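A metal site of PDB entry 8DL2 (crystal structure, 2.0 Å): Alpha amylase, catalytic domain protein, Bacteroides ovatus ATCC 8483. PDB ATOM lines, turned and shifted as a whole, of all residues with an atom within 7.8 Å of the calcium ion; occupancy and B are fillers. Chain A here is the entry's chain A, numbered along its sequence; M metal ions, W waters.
The side-chain hydroxyl of Tyr 269 lies close to the side-chain carboxylate of Glu 336.
OG of Ser 356 is in hydrogen-bond range of OD1 of Asp 354 (2.6 Å).
The backbone carbonyl oxygen (O) of Glu 336 sits at hydrogen-bond distance from the backbone NH (N) of Gly 348 (2.8 Å).
N of Glu 254 lies within hydrogen-bond range of OD2 of Asp 258.
Of the 21 residues printed, 5 come within 4 Å of the calcium ion.
The nearest printed residue that does not touch the calcium ion is Ala 338 (4.2 Å).
The calcium ion is bound by the side-chain carboxylate of Glu 336, the backbone carbonyl oxygen of Phe 337, the side-chain carboxylate of Asp 354, the side-chain carboxylate of Glu 254, water W1 and the backbone carbonyl oxygen of Gly 339.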
ATOM      1  N   ALA A 252       3.461   4.214  19.611  1.00  0.00           N
ATOM      2  CA  ALA A 252       3.907   5.475  20.228  1.00  0.00           C
ATOM      3  C   ALA A 252       5.398   5.680  19.916  1.00  0.00           C
ATOM      4  O   ALA A 252       6.107   4.711  19.679  1.00  0.00           O
ATOM      5  CB  ALA A 252       3.643   5.429  21.713  1.00  0.00           C
ATOM      6  N   LEU A 253       5.811   6.943  19.889  1.00  0.00           N
ATOM      7  CA  LEU A 253       7.233   7.288  19.865  1.00  0.00           C
ATOM      8  C   LEU A 253       7.577   7.867  21.235  1.00  0.00           C
ATOM      9  O   LEU A 253       6.783   8.657  21.800  1.00  0.00           O
ATOM     10  CB  LEU A 253       7.491   8.324  18.766  1.00  0.00           C
ATOM     11  CG  LEU A 253       6.989   7.997  17.356  1.00  0.00           C
ATOM     12  CD1 LEU A 253       7.294   9.193  16.460  1.00  0.00           C
ATOM     13  CD2 LEU A 253       7.642   6.736  16.806  1.00  0.00           C
ATOM     14  N   GLU A 254       8.768   7.505  21.710  1.00  0.00           N
ATOM     15  CA  GLU A 254       9.263   7.831  23.057  1.00  0.00           C
ATOM     16  C   GLU A 254      10.479   8.742  22.917  1.00  0.00           C
ATOM     17  O   GLU A 254      11.437   8.339  22.268  1.00  0.00           O
ATOM     18  CB  GLU A 254       9.561   6.528  23.786  1.00  0.00           C
ATOM     19  CG  GLU A 254       9.773   6.787  25.253  1.00  0.00           C
ATOM     20  CD  GLU A 254      10.280   5.630  26.108  1.00  0.00           C
ATOM     21  OE1 GLU A 254      10.208   4.445  25.675  1.00  0.00           O
ATOM     22  OE2 GLU A 254      10.705   5.958  27.256  1.00  0.00           O
ATOM     23  N   VAL A 257      14.350   7.581  22.916  1.00  0.00           N
ATOM     24  CA  VAL A 257      14.492   6.227  22.316  1.00  0.00           C
ATOM     25  C   VAL A 257      14.338   6.374  20.800  1.00  0.00           C
ATOM     26  O   VAL A 257      15.206   5.906  20.067  1.00  0.00           O
ATOM     27  CB  VAL A 257      13.480   5.219  22.882  1.00  0.00           C
ATOM     28  CG1 VAL A 257      13.567   3.877  22.170  1.00  0.00           C
ATOM     29  CG2 VAL A 257      13.660   5.039  24.385  1.00  0.00           C
ATOM     30  N   ASP A 258      13.236   6.981  20.377  1.00  0.00           N
ATOM     31  CA  ASP A 258      12.926   7.140  18.931  1.00  0.00           C
ATOM     32  C   ASP A 258      13.660   8.402  18.445  1.00  0.00           C
ATOM     33  O   ASP A 258      13.384   9.484  18.978  1.00  0.00           O
ATOM     34  CB  ASP A 258      11.405   7.080  18.760  1.00  0.00           C
ATOM     35  CG  ASP A 258      10.869   5.702  19.128  1.00  0.00           C
ATOM     36  OD1 ASP A 258      11.280   4.718  18.480  1.00  0.00           O
ATOM     37  OD2 ASP A 258      10.105   5.584  20.118  1.00  0.00           O
ATOM     38  N   TYR A 269       5.799  10.933  25.218  1.00  0.00           N
ATOM     39  CA  TYR A 269       5.150  10.072  24.220  1.00  0.00           C
ATOM     40  C   TYR A 269       4.271  10.894  23.264  1.00  0.00           C
ATOM     41  O   TYR A 269       3.535  11.798  23.693  1.00  0.00           O
ATOM     42  CB  TYR A 269       4.239   9.007  24.851  1.00  0.00           C
ATOM     43  CG  TYR A 269       4.924   7.854  25.544  1.00  0.00           C
ATOM     44  CD1 TYR A 269       5.733   6.970  24.846  1.00  0.00           C
ATOM     45  CD2 TYR A 269       4.694   7.582  26.884  1.00  0.00           C
ATOM     46  CE1 TYR A 269       6.338   5.882  25.466  1.00  0.00           C
ATOM     47  CE2 TYR A 269       5.270   6.487  27.519  1.00  0.00           C
ATOM     48  CZ  TYR A 269       6.124   5.639  26.806  1.00  0.00           C
ATOM     49  OH  TYR A 269       6.693   4.544  27.392  1.00  0.00           O
ATOM     50  N   GLN A 335       4.580  -4.718  27.322  1.00  0.00           N
ATOM     51  CA  GLN A 335       3.868  -3.434  27.129  1.00  0.00           C
ATOM     52  C   GLN A 335       4.889  -2.285  27.226  1.00  0.00           C
ATOM     53  O   GLN A 335       5.863  -2.405  27.972  1.00  0.00           O
ATOM     54  CB  GLN A 335       2.687  -3.351  28.080  1.00  0.00           C
ATOM     55  CG  GLN A 335       1.593  -4.349  27.684  1.00  0.00           C
ATOM     56  CD  GLN A 335       0.712  -4.696  28.848  1.00  0.00           C
ATOM     57  OE1 GLN A 335       1.121  -5.353  29.786  1.00  0.00           O
ATOM     58  NE2 GLN A 335      -0.515  -4.224  28.810  1.00  0.00           N
ATOM     59  N   GLU A 336       4.678  -1.240  26.437  1.00  0.00           N
ATOM     60  CA  GLU A 336       5.554  -0.042  26.369  1.00  0.00           C
ATOM     61  C   GLU A 336       6.039   0.346  27.785  1.00  0.00           C
ATOM     62  O   GLU A 336       5.231   0.761  28.611  1.00  0.00           O
ATOM     63  CB  GLU A 336       4.774   1.067  25.670  1.00  0.00           C
ATOM     64  CG  GLU A 336       5.510   2.375  25.565  1.00  0.00           C
ATOM     65  CD  GLU A 336       6.927   2.341  25.003  1.00  0.00           C
ATOM     66  OE1 GLU A 336       7.154   1.725  23.953  1.00  0.00           O
ATOM     67  OE2 GLU A 336       7.804   2.908  25.660  1.00  0.00           O
ATOM     68  N   PHE A 337       7.327   0.225  28.038  1.00  0.00           N
ATOM     69  CA  PHE A 337       8.027   0.535  29.307  1.00  0.00           C
ATOM     70  C   PHE A 337       8.993   1.703  29.106  1.00  0.00           C
ATOM     71  O   PHE A 337       9.399   1.965  27.970  1.00  0.00           O
ATOM     72  CB  PHE A 337       8.726  -0.722  29.838  1.00  0.00           C
ATOM     73  CG  PHE A 337       9.541  -1.531  28.871  1.00  0.00           C
ATOM     74  CD1 PHE A 337      10.773  -1.098  28.434  1.00  0.00           C
ATOM     75  CD2 PHE A 337       9.084  -2.738  28.395  1.00  0.00           C
ATOM     76  CE1 PHE A 337      11.528  -1.851  27.543  1.00  0.00           C
ATOM     77  CE2 PHE A 337       9.846  -3.501  27.511  1.00  0.00           C
ATOM     78  CZ  PHE A 337      11.078  -3.068  27.089  1.00  0.00           C
ATOM     79  N   ALA A 338       9.379   2.364  30.199  1.00  0.00           N
ATOM     80  CA  ALA A 338      10.289   3.540  30.195  1.00  0.00           C
ATOM     81  C   ALA A 338      11.613   3.110  29.547  1.00  0.00           C
ATOM     82  O   ALA A 338      12.196   2.092  30.011  1.00  0.00           O
ATOM     83  CB  ALA A 338      10.497   4.109  31.586  1.00  0.00           C
ATOM     84  N   GLY A 339      12.003   3.816  28.468  1.00  0.00           N
ATOM     85  CA  GLY A 339      13.240   3.541  27.733  1.00  0.00           C
ATOM     86  C   GLY A 339      13.216   2.237  26.963  1.00  0.00           C
ATOM     87  O   GLY A 339      12.141   1.778  26.565  1.00  0.00           O
ATOM     88  N   ASN A 340      14.385   1.634  26.713  1.00  0.00           N
ATOM     89  CA  ASN A 340      14.490   0.439  25.849  1.00  0.00           C
ATOM     90  C   ASN A 340      15.433  -0.594  26.477  1.00  0.00           C
ATOM     91  O   ASN A 340      15.948  -1.416  25.749  1.00  0.00           O
ATOM     92  CB  ASN A 340      14.959   0.862  24.464  1.00  0.00           C
ATOM     93  CG  ASN A 340      16.333   1.513  24.492  1.00  0.00           C
ATOM     94  OD1 ASN A 340      16.965   1.664  25.537  1.00  0.00           O
ATOM     95  ND2 ASN A 340      16.818   1.879  23.327  1.00  0.00           N
ATOM     96  N   ASP A 341      15.704  -0.512  27.777  1.00  0.00           N
ATOM     97  CA  ASP A 341      16.619  -1.431  28.509  1.00  0.00           C
ATOM     98  C   ASP A 341      15.997  -1.723  29.884  1.00  0.00           C
ATOM     99  O   ASP A 341      16.208  -0.941  30.834  1.00  0.00           O
ATOM    100  CB  ASP A 341      18.005  -0.809  28.678  1.00  0.00           C
ATOM    101  CG  ASP A 341      18.963  -1.710  29.424  1.00  0.00           C
ATOM    102  OD1 ASP A 341      18.518  -2.813  29.858  1.00  0.00           O
ATOM    103  OD2 ASP A 341      20.148  -1.315  29.554  1.00  0.00           O
ATOM    104  N   SER A 342      15.230  -2.787  30.006  1.00  0.00           N
ATOM    105  CA  SER A 342      14.340  -2.973  31.175  1.00  0.00           C
ATOM    106  C   SER A 342      13.912  -4.433  31.276  1.00  0.00           C
ATOM    107  O   SER A 342      13.734  -5.069  30.232  1.00  0.00           O
ATOM    108  CB  SER A 342      13.172  -1.995  31.036  1.00  0.00           C
ATOM    109  OG  SER A 342      12.249  -2.070  32.089  1.00  0.00           O
ATOM    110  N   ASN A 346       7.725  -1.384  34.472  1.00  0.00           N
ATOM    111  CA  ASN A 346       7.722   0.101  34.462  1.00  0.00           C
ATOM    112  C   ASN A 346       6.900   0.533  33.244  1.00  0.00           C
ATOM    113  O   ASN A 346       7.428   1.201  32.364  1.00  0.00           O
ATOM    114  CB  ASN A 346       9.150   0.616  34.442  1.00  0.00           C
ATOM    115  CG  ASN A 346       9.287   2.096  34.771  1.00  0.00           C
ATOM    116  OD1 ASN A 346       8.309   2.785  35.076  1.00  0.00           O
ATOM    117  ND2 ASN A 346      10.510   2.605  34.674  1.00  0.00           N
ATOM    118  N   GLY A 348       4.487   2.397  30.810  1.00  0.00           N
ATOM    119  CA  GLY A 348       3.964   3.744  30.490  1.00  0.00           C
ATOM    120  C   GLY A 348       2.695   3.705  29.660  1.00  0.00           C
ATOM    121  O   GLY A 348       1.840   4.613  29.813  1.00  0.00           O
ATOM    122  N   LEU A 353       2.790  -2.117  22.508  1.00  0.00           N
ATOM    123  CA  LEU A 353       3.906  -3.015  22.929  1.00  0.00           C
ATOM    124  C   LEU A 353       5.233  -2.336  22.637  1.00  0.00           C
ATOM    125  O   LEU A 353       5.304  -1.525  21.669  1.00  0.00           O
ATOM    126  CB  LEU A 353       3.794  -4.362  22.215  1.00  0.00           C
ATOM    127  CG  LEU A 353       2.509  -5.135  22.473  1.00  0.00           C
ATOM    128  CD1 LEU A 353       2.713  -6.599  22.173  1.00  0.00           C
ATOM    129  CD2 LEU A 353       1.965  -4.951  23.898  1.00  0.00           C
ATOM    130  N   ASP A 354       6.247  -2.589  23.450  1.00  0.00           N
ATOM    131  CA  ASP A 354       7.529  -1.854  23.320  1.00  0.00           C
ATOM    132  C   ASP A 354       8.130  -2.132  21.933  1.00  0.00           C
ATOM    133  O   ASP A 354       8.363  -3.299  21.564  1.00  0.00           O
ATOM    134  CB  ASP A 354       8.466  -2.074  24.521  1.00  0.00           C
ATOM    135  CG  ASP A 354       9.451  -0.932  24.638  1.00  0.00           C
ATOM    136  OD1 ASP A 354      10.409  -0.956  23.842  1.00  0.00           O
ATOM    137  OD2 ASP A 354       9.249   0.019  25.457  1.00  0.00           O
ATOM    138  N   ALA A 355       8.430  -1.073  21.202  1.00  0.00           N
ATOM    139  CA  ALA A 355       8.974  -1.166  19.825  1.00  0.00           C
ATOM    140  C   ALA A 355      10.437  -1.615  19.871  1.00  0.00           C
ATOM    141  O   ALA A 355      10.915  -2.099  18.848  1.00  0.00           O
ATOM    142  CB  ALA A 355       8.798   0.148  19.075  1.00  0.00           C
ATOM    143  N   SER A 356      11.104  -1.555  21.045  1.00  0.00           N
ATOM    144  CA  SER A 356      12.491  -2.057  21.191  1.00  0.00           C
ATOM    145  C   SER A 356      12.550  -3.570  20.933  1.00  0.00           C
ATOM    146  O   SER A 356      13.621  -4.057  20.548  1.00  0.00           O
ATOM    147  CB  SER A 356      13.086  -1.718  22.537  1.00  0.00           C
ATOM    148  OG  SER A 356      12.480  -2.478  23.588  1.00  0.00           O
ATOM    149  N   ASP A 389       5.001   8.753  32.976  1.00  0.00           N
ATOM    150  CA  ASP A 389       4.798   9.005  31.528  1.00  0.00           C
ATOM    151  C   ASP A 389       3.371   8.672  31.092  1.00  0.00           C
ATOM    152  O   ASP A 389       2.993   9.174  30.030  1.00  0.00           O
ATOM    153  CB  ASP A 389       5.741   8.198  30.631  1.00  0.00           C
ATOM    154  CG  ASP A 389       7.205   8.445  30.927  1.00  0.00           C
ATOM    155  OD1 ASP A 389       7.555   9.550  31.405  1.00  0.00           O
ATOM    156  OD2 ASP A 389       7.988   7.530  30.661  1.00  0.00           O
HETATM  157 CA    CA M   1       9.904   2.172  25.790  1.00  0.00          CA
HETATM  158  O   HOH W   1      10.867   1.585  23.687  1.00  0.00           O
